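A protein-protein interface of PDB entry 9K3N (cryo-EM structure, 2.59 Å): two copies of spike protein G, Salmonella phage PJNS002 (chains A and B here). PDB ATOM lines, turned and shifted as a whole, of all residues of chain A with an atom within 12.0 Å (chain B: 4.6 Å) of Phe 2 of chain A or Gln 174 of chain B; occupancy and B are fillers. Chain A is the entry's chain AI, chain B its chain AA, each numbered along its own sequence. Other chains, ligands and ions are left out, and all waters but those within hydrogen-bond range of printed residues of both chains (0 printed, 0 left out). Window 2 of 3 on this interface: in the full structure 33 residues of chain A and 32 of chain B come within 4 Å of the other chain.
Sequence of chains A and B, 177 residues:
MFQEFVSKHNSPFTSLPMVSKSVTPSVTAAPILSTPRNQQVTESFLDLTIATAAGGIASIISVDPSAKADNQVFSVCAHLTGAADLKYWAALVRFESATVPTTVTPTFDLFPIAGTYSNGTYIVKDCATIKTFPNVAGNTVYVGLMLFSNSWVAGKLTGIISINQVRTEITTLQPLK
Phe 2 of chain A touches just these residues of chain B: Phe 5 (3.1 Å), Val 6 (3.9 Å), Ser 7 (2.8 Å), Asn 10 (3.9 Å) and Gln 174 (3.4 Å).
Of chain A, only Phe 2 (3.4 Å) comes within 4 Å of Gln 174 of chain B.
Of the printed residues of chain A, Val 6 of chain B touches Phe 2 (3.9 Å), Gln 3 (3.98 Å) and Glu 4 (2.8 Å).
Of the printed residues of chain A, Ser 7 of chain B touches Met 1, Phe 2, Gln 3 and Glu 4.
No residue of chain A comes within 4 Å of Thr 172 of chain B.
No residue of chain A comes within 4 Å of Leu 176 of chain B.
No residue of chain A comes within 4 Å of Lys 177 of chain B.
Of the printed residues of chain B, Phe 5 of chain A touches Glu 169 (3.8 Å).
Printed residues of chain B within 4 Å of Met 1 of chain A: Phe 5 (3.9 Å), Ser 7 (3.8 Å) and Asn 10 (3.3 Å).
Printed residues of chain B within 4 Å of Gln 3 of chain A: Val 6 (3.98 Å), Ser 7 (3.6 Å) and Asn 10 (3.6 Å).
Of the printed residues of chain A, Asn 10 of chain B touches Met 1 (3.3 Å), Phe 2 (3.9 Å) and Gln 3 (3.6 Å).
Of the printed residues of chain B, Pro 175 of chain A touches Glu 169.
The nearest residue of chain B that does not touch Phe 2 of chain A is Glu 169 of chain B (4.3 Å).
The nearest printed residue of chain A that does not touch Asn 10 of chain B is Glu 4 of chain A (6.2 Å).
Among the printed residues, pairs that only touch across the chains: Met 1 of chain A with Phe 5 of chain B (3.9 Å), Met 1 of chain A with Ser 7 of chain B (3.8 Å), Phe 2 of chain A with Val 6 of chain B (3.9 Å), Phe 2 of chain A with Asn 10 of chain B (3.9 Å), Phe 2 of chain A with Gln 174 of chain B (3.4 Å), Gln 3 of chain A with Val 6 of chain B (3.98 Å), Gln 3 of chain A with Ser 7 of chain B (3.6 Å), Gln 3 of chain A with Asn 10 of chain B (3.6 Å), Glu 4 of chain A with Val 6 of chain B (2.8 Å), Phe 5 of chain A with Glu 169 of chain B (3.8 Å), Pro 175 of chain A with Glu 169 of chain B (3.3 Å) and Leu 176 of chain A with Glu 169 of chain B (3.8 Å).
The backbone NH (N) of Phe 2 of chain A lies close to the backbone carbonyl oxygen (O) of Phe 5 of chain B, at 3.2 Å.
N of Ser 7 of chain B sits at hydrogen-bond distance from O of Phe 2 of chain A, at 3.1 Å.
The backbone NH (N) of Glu 4 of chain A is in hydrogen-bond range of the backbone carbonyl oxygen (O) of Ser 7 of chain B (3.5 Å).
N of Met 1 of chain A lies within hydrogen-bond range of OD1 of Asn 10 of chain B, at 3.3 Å.
Positions printed for both chains: 5, 6, 172, 173, 174, 175, 176 and 177.
Of the 16 pairs that touch across the chains among the printed residues, none has its exchanged pair printed and touching as well.
Of the 12 printed residues of chain A, 7 touch a printed residue of chain B.
Printed residues of chain B that touch a printed residue of chain A: Phe 5, Val 6, Ser 7, Asn 10, Glu 169 and Gln 174.
Hydrophobic or aromatic side chains of chain B that line the printed part of chain A: Val 6.
The side-chain amide oxygen (OE1) of Gln 174 of chain B lies within hydrogen-bond range of the side-chain amino group (NZ) of Lys 177 of chain B (2.8 Å).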
ATOM      1  N   MET A   1     -22.443  -4.620 -14.904  1.00  0.00           N
ATOM      2  CA  MET A   1     -21.567  -3.923 -13.970  1.00  0.00           C
ATOM      3  C   MET A   1     -20.688  -2.908 -14.694  1.00  0.00           C
ATOM      4  O   MET A   1     -20.708  -2.822 -15.921  1.00  0.00           O
ATOM      5  CB  MET A   1     -20.699  -4.923 -13.201  1.00  0.00           C
ATOM      6  CG  MET A   1     -21.483  -5.849 -12.282  1.00  0.00           C
ATOM      7  SD  MET A   1     -20.432  -6.873 -11.232  1.00  0.00           S
ATOM      8  CE  MET A   1     -20.543  -8.453 -12.064  1.00  0.00           C
ATOM      9  N   PHE A   2     -19.920  -2.138 -13.929  1.00  0.00           N
ATOM     10  CA  PHE A   2     -19.004  -1.159 -14.489  1.00  0.00           C
ATOM     11  C   PHE A   2     -17.644  -1.796 -14.761  1.00  0.00           C
ATOM     12  O   PHE A   2     -17.281  -2.822 -14.182  1.00  0.00           O
ATOM     13  CB  PHE A   2     -18.839   0.034 -13.548  1.00  0.00           C
ATOM     14  CG  PHE A   2     -20.114   0.780 -13.277  1.00  0.00           C
ATOM     15  CD1 PHE A   2     -20.580   1.732 -14.168  1.00  0.00           C
ATOM     16  CD2 PHE A   2     -20.844   0.539 -12.125  1.00  0.00           C
ATOM     17  CE1 PHE A   2     -21.752   2.424 -13.919  1.00  0.00           C
ATOM     18  CE2 PHE A   2     -22.016   1.227 -11.870  1.00  0.00           C
ATOM     19  CZ  PHE A   2     -22.469   2.171 -12.768  1.00  0.00           C
ATOM     20  N   GLN A   3     -16.890  -1.168 -15.659  1.00  0.00           N
ATOM     21  CA  GLN A   3     -15.527  -1.599 -15.938  1.00  0.00           C
ATOM     22  C   GLN A   3     -14.562  -1.014 -14.914  1.00  0.00           C
ATOM     23  O   GLN A   3     -14.787   0.066 -14.359  1.00  0.00           O
ATOM     24  CB  GLN A   3     -15.105  -1.188 -17.348  1.00  0.00           C
ATOM     25  CG  GLN A   3     -15.233  -2.295 -18.380  1.00  0.00           C
ATOM     26  CD  GLN A   3     -14.257  -3.433 -18.139  1.00  0.00           C
ATOM     27  OE1 GLN A   3     -13.130  -3.215 -17.701  1.00  0.00           O
ATOM     28  NE2 GLN A   3     -14.693  -4.653 -18.419  1.00  0.00           N
ATOM     29  N   GLU A   4     -13.529  -1.747 -14.557  1.00  0.00           N
ATOM     30  CA  GLU A   4     -12.456  -1.205 -13.760  1.00  0.00           C
ATOM     31  C   GLU A   4     -11.519  -0.637 -14.819  1.00  0.00           C
ATOM     32  O   GLU A   4     -11.008  -1.337 -15.628  1.00  0.00           O
ATOM     33  CB  GLU A   4     -11.900  -2.297 -12.850  1.00  0.00           C
ATOM     34  CG  GLU A   4     -10.820  -1.794 -11.928  1.00  0.00           C
ATOM     35  CD  GLU A   4     -11.362  -0.782 -10.946  1.00  0.00           C
ATOM     36  OE1 GLU A   4     -12.586  -0.679 -10.838  1.00  0.00           O
ATOM     37  OE2 GLU A   4     -10.572  -0.068 -10.288  1.00  0.00           O
ATOM     38  N   PHE A   5     -11.454   0.687 -14.878  1.00  0.00           N
ATOM     39  CA  PHE A   5     -10.465   1.336 -15.723  1.00  0.00           C
ATOM     40  C   PHE A   5      -9.165   1.627 -14.983  1.00  0.00           C
ATOM     41  O   PHE A   5      -8.455   2.567 -15.338  1.00  0.00           O
ATOM     42  CB  PHE A   5     -11.034   2.643 -16.282  1.00  0.00           C
ATOM     43  CG  PHE A   5     -11.956   2.453 -17.450  1.00  0.00           C
ATOM     44  CD1 PHE A   5     -11.453   2.336 -18.734  1.00  0.00           C
ATOM     45  CD2 PHE A   5     -13.326   2.393 -17.264  1.00  0.00           C
ATOM     46  CE1 PHE A   5     -12.298   2.162 -19.812  1.00  0.00           C
ATOM     47  CE2 PHE A   5     -14.177   2.220 -18.340  1.00  0.00           C
ATOM     48  CZ  PHE A   5     -13.663   2.104 -19.617  1.00  0.00           C
ATOM     49  N   VAL A   6      -8.837   0.841 -13.960  1.00  0.00           N
ATOM     50  CA  VAL A   6      -7.641   1.157 -13.187  1.00  0.00           C
ATOM     51  C   VAL A   6      -6.845  -0.126 -13.009  1.00  0.00           C
ATOM     52  O   VAL A   6      -7.387  -1.141 -12.560  1.00  0.00           O
ATOM     53  CB  VAL A   6      -7.988   1.782 -11.823  1.00  0.00           C
ATOM     54  CG1 VAL A   6      -6.723   2.029 -11.017  1.00  0.00           C
ATOM     55  CG2 VAL A   6      -8.762   3.076 -12.011  1.00  0.00           C
ATOM     56  N   THR A 172      -7.444   5.376 -22.671  1.00  0.00           N
ATOM     57  CA  THR A 172      -8.231   4.296 -23.247  1.00  0.00           C
ATOM     58  C   THR A 172      -9.654   4.788 -23.474  1.00  0.00           C
ATOM     59  O   THR A 172     -10.059   5.841 -22.976  1.00  0.00           O
ATOM     60  CB  THR A 172      -8.226   3.050 -22.351  1.00  0.00           C
ATOM     61  OG1 THR A 172      -8.919   1.984 -23.010  1.00  0.00           O
ATOM     62  CG2 THR A 172      -8.907   3.343 -21.023  1.00  0.00           C
ATOM     63  N   LEU A 173     -10.413   4.009 -24.239  1.00  0.00           N
ATOM     64  CA  LEU A 173     -11.784   4.372 -24.578  1.00  0.00           C
ATOM     65  C   LEU A 173     -12.706   4.108 -23.394  1.00  0.00           C
ATOM     66  O   LEU A 173     -12.809   2.970 -22.924  1.00  0.00           O
ATOM     67  CB  LEU A 173     -12.253   3.592 -25.805  1.00  0.00           C
ATOM     68  CG  LEU A 173     -13.741   3.720 -26.141  1.00  0.00           C
ATOM     69  CD1 LEU A 173     -14.092   5.149 -26.521  1.00  0.00           C
ATOM     70  CD2 LEU A 173     -14.131   2.754 -27.247  1.00  0.00           C
ATOM     71  N   GLN A 174     -13.370   5.155 -22.915  1.00  0.00           N
ATOM     72  CA  GLN A 174     -14.400   5.025 -21.895  1.00  0.00           C
ATOM     73  C   GLN A 174     -15.743   5.392 -22.509  1.00  0.00           C
ATOM     74  O   GLN A 174     -15.984   6.575 -22.793  1.00  0.00           O
ATOM     75  CB  GLN A 174     -14.098   5.916 -20.689  1.00  0.00           C
ATOM     76  CG  GLN A 174     -12.794   5.581 -19.983  1.00  0.00           C
ATOM     77  CD  GLN A 174     -12.602   6.372 -18.704  1.00  0.00           C
ATOM     78  OE1 GLN A 174     -11.656   7.149 -18.577  1.00  0.00           O
ATOM     79  NE2 GLN A 174     -13.498   6.173 -17.747  1.00  0.00           N
ATOM     80  N   PRO A 175     -16.638   4.427 -22.740  1.00  0.00           N
ATOM     81  CA  PRO A 175     -17.878   4.727 -23.477  1.00  0.00           C
ATOM     82  C   PRO A 175     -18.778   5.754 -22.809  1.00  0.00           C
ATOM     83  O   PRO A 175     -19.579   6.389 -23.504  1.00  0.00           O
ATOM     84  CB  PRO A 175     -18.568   3.359 -23.572  1.00  0.00           C
ATOM     85  CG  PRO A 175     -17.463   2.366 -23.410  1.00  0.00           C
ATOM     86  CD  PRO A 175     -16.496   2.990 -22.455  1.00  0.00           C
ATOM     87  N   LEU A 176     -18.683   5.939 -21.492  1.00  0.00           N
ATOM     88  CA  LEU A 176     -19.552   6.877 -20.796  1.00  0.00           C
ATOM     89  C   LEU A 176     -18.991   8.292 -20.738  1.00  0.00           C
ATOM     90  O   LEU A 176     -19.694   9.197 -20.279  1.00  0.00           O
ATOM     91  CB  LEU A 176     -19.832   6.381 -19.372  1.00  0.00           C
ATOM     92  CG  LEU A 176     -20.645   5.090 -19.251  1.00  0.00           C
ATOM     93  CD1 LEU A 176     -20.872   4.732 -17.790  1.00  0.00           C
ATOM     94  CD2 LEU A 176     -21.969   5.211 -19.990  1.00  0.00           C
ATOM     95  N   LYS A 177     -17.758   8.507 -21.183  1.00  0.00           N
ATOM     96  CA  LYS A 177     -17.156   9.829 -21.086  1.00  0.00           C
ATOM     97  C   LYS A 177     -17.854  10.809 -22.020  1.00  0.00           C
ATOM     98  O   LYS A 177     -18.491  11.761 -21.569  1.00  0.00           O
ATOM     99  CB  LYS A 177     -15.664   9.777 -21.406  1.00  0.00           C
ATOM    100  CG  LYS A 177     -14.799   9.240 -20.278  1.00  0.00           C
ATOM    101  CD  LYS A 177     -15.071   9.975 -18.976  1.00  0.00           C
ATOM    102  CE  LYS A 177     -14.134   9.507 -17.874  1.00  0.00           C
ATOM    103  NZ  LYS A 177     -12.704   9.771 -18.198  1.00  0.00           N
ATOM    104  N   PHE B   5     -20.277  -2.833  -7.248  1.00  0.00           N
ATOM    105  CA  PHE B   5     -20.773  -2.788  -8.614  1.00  0.00           C
ATOM    106  C   PHE B   5     -19.659  -2.585  -9.635  1.00  0.00           C
ATOM    107  O   PHE B   5     -19.906  -2.037 -10.708  1.00  0.00           O
ATOM    108  CB  PHE B   5     -21.805  -1.668  -8.758  1.00  0.00           C
ATOM    109  CG  PHE B   5     -23.166  -2.025  -8.239  1.00  0.00           C
ATOM    110  CD1 PHE B   5     -24.068  -2.708  -9.036  1.00  0.00           C
ATOM    111  CD2 PHE B   5     -23.546  -1.676  -6.955  1.00  0.00           C
ATOM    112  CE1 PHE B   5     -25.324  -3.037  -8.563  1.00  0.00           C
ATOM    113  CE2 PHE B   5     -24.800  -2.003  -6.476  1.00  0.00           C
ATOM    114  CZ  PHE B   5     -25.691  -2.685  -7.281  1.00  0.00           C
ATOM    115  N   VAL B   6     -18.438  -3.014  -9.324  1.00  0.00           N
ATOM    116  CA  VAL B   6     -17.345  -2.750 -10.252  1.00  0.00           C
ATOM    117  C   VAL B   6     -16.562  -4.041 -10.435  1.00  0.00           C
ATOM    118  O   VAL B   6     -16.148  -4.665  -9.453  1.00  0.00           O
ATOM    119  CB  VAL B   6     -16.427  -1.619  -9.750  1.00  0.00           C
ATOM    120  CG1 VAL B   6     -15.259  -1.422 -10.703  1.00  0.00           C
ATOM    121  CG2 VAL B   6     -17.212  -0.327  -9.594  1.00  0.00           C
ATOM    122  N   SER B   7     -16.361  -4.438 -11.688  1.00  0.00           N
ATOM    123  CA  SER B   7     -15.711  -5.708 -11.969  1.00  0.00           C
ATOM    124  C   SER B   7     -14.965  -5.626 -13.291  1.00  0.00           C
ATOM    125  O   SER B   7     -15.208  -4.738 -14.114  1.00  0.00           O
ATOM    126  CB  SER B   7     -16.723  -6.861 -12.009  1.00  0.00           C
ATOM    127  OG  SER B   7     -16.105  -8.064 -12.433  1.00  0.00           O
ATOM    128  N   ASN B  10     -16.836  -8.129 -17.757  1.00  0.00           N
ATOM    129  CA  ASN B  10     -18.259  -8.391 -17.920  1.00  0.00           C
ATOM    130  C   ASN B  10     -18.457  -9.441 -19.007  1.00  0.00           C
ATOM    131  O   ASN B  10     -17.861  -9.362 -20.086  1.00  0.00           O
ATOM    132  CB  ASN B  10     -19.006  -7.105 -18.265  1.00  0.00           C
ATOM    133  CG  ASN B  10     -19.000  -6.107 -17.127  1.00  0.00           C
ATOM    134  OD1 ASN B  10     -19.830  -6.177 -16.223  1.00  0.00           O
ATOM    135  ND2 ASN B  10     -18.058  -5.172 -17.164  1.00  0.00           N
ATOM    136  N   GLU B 169     -20.620  -0.382 -22.603  1.00  0.00           N
ATOM    137  CA  GLU B 169     -20.714  -0.794 -21.214  1.00  0.00           C
ATOM    138  C   GLU B 169     -22.109  -1.324 -20.922  1.00  0.00           C
ATOM    139  O   GLU B 169     -23.078  -0.989 -21.609  1.00  0.00           O
ATOM    140  CB  GLU B 169     -20.375   0.357 -20.258  1.00  0.00           C
ATOM    141  CG  GLU B 169     -18.962   0.893 -20.422  1.00  0.00           C
ATOM    142  CD  GLU B 169     -18.503   1.712 -19.232  1.00  0.00           C
ATOM    143  OE1 GLU B 169     -18.887   1.375 -18.092  1.00  0.00           O
ATOM    144  OE2 GLU B 169     -17.760   2.694 -19.439  1.00  0.00           O
ATOM    145  N   THR B 172     -26.629  -2.340 -14.877  1.00  0.00           N
ATOM    146  CA  THR B 172     -27.205  -3.324 -13.973  1.00  0.00           C
ATOM    147  C   THR B 172     -28.098  -2.611 -12.968  1.00  0.00           C
ATOM    148  O   THR B 172     -28.071  -1.384 -12.838  1.00  0.00           O
ATOM    149  CB  THR B 172     -26.119  -4.134 -13.251  1.00  0.00           C
ATOM    150  OG1 THR B 172     -26.732  -5.158 -12.461  1.00  0.00           O
ATOM    151  CG2 THR B 172     -25.292  -3.231 -12.347  1.00  0.00           C
ATOM    152  N   LEU B 173     -28.900  -3.397 -12.255  1.00  0.00           N
ATOM    153  CA  LEU B 173     -29.842  -2.852 -11.285  1.00  0.00           C
ATOM    154  C   LEU B 173     -29.108  -2.446 -10.013  1.00  0.00           C
ATOM    155  O   LEU B 173     -28.468  -3.281  -9.366  1.00  0.00           O
ATOM    156  CB  LEU B 173     -30.932  -3.874 -10.970  1.00  0.00           C
ATOM    157  CG  LEU B 173     -31.865  -3.511  -9.811  1.00  0.00           C
ATOM    158  CD1 LEU B 173     -32.677  -2.269 -10.135  1.00  0.00           C
ATOM    159  CD2 LEU B 173     -32.773  -4.679  -9.460  1.00  0.00           C
ATOM    160  N   GLN B 174     -29.202  -1.168  -9.659  1.00  0.00           N
ATOM    161  CA  GLN B 174     -28.689  -0.672  -8.389  1.00  0.00           C
ATOM    162  C   GLN B 174     -29.863  -0.226  -7.529  1.00  0.00           C
ATOM    163  O   GLN B 174     -30.489   0.801  -7.831  1.00  0.00           O
ATOM    164  CB  GLN B 174     -27.711   0.485  -8.604  1.00  0.00           C
ATOM    165  CG  GLN B 174     -26.478   0.111  -9.412  1.00  0.00           C
ATOM    166  CD  GLN B 174     -25.457   1.229  -9.470  1.00  0.00           C
ATOM    167  OE1 GLN B 174     -25.142   1.742 -10.544  1.00  0.00           O
ATOM    168  NE2 GLN B 174     -24.929   1.608  -8.314  1.00  0.00           N
ATOM    169  N   PRO B 175     -30.204  -0.960  -6.466  1.00  0.00           N
ATOM    170  CA  PRO B 175     -31.430  -0.644  -5.710  1.00  0.00           C
ATOM    171  C   PRO B 175     -31.445   0.740  -5.082  1.00  0.00           C
ATOM    172  O   PRO B 175     -32.534   1.265  -4.820  1.00  0.00           O
ATOM    173  CB  PRO B 175     -31.471  -1.743  -4.639  1.00  0.00           C
ATOM    174  CG  PRO B 175     -30.646  -2.854  -5.202  1.00  0.00           C
ATOM    175  CD  PRO B 175     -29.557  -2.191  -5.984  1.00  0.00           C
ATOM    176  N   LEU B 176     -30.288   1.348  -4.824  1.00  0.00           N
ATOM    177  CA  LEU B 176     -30.247   2.654  -4.183  1.00  0.00           C
ATOM    178  C   LEU B 176     -30.299   3.814  -5.169  1.00  0.00           C
ATOM    179  O   LEU B 176     -30.392   4.966  -4.734  1.00  0.00           O
ATOM    180  CB  LEU B 176     -28.987   2.779  -3.317  1.00  0.00           C
ATOM    181  CG  LEU B 176     -28.907   1.856  -2.100  1.00  0.00           C
ATOM    182  CD1 LEU B 176     -27.626   2.105  -1.319  1.00  0.00           C
ATOM    183  CD2 LEU B 176     -30.124   2.030  -1.206  1.00  0.00           C
ATOM    184  N   LYS B 177     -30.243   3.547  -6.469  1.00  0.00           N
ATOM    185  CA  LYS B 177     -30.222   4.628  -7.446  1.00  0.00           C
ATOM    186  C   LYS B 177     -31.561   5.354  -7.474  1.00  0.00           C
ATOM    187  O   LYS B 177     -31.645   6.529  -7.118  1.00  0.00           O
ATOM    188  CB  LYS B 177     -29.885   4.101  -8.838  1.00  0.00           C
ATOM    189  CG  LYS B 177     -28.413   3.802  -9.058  1.00  0.00           C
ATOM    190  CD  LYS B 177     -27.546   4.992  -8.682  1.00  0.00           C
ATOM    191  CE  LYS B 177     -26.082   4.729  -8.997  1.00  0.00           C
ATOM    192  NZ  LYS B 177     -25.849   4.500 -10.450  1.00  0.00           N
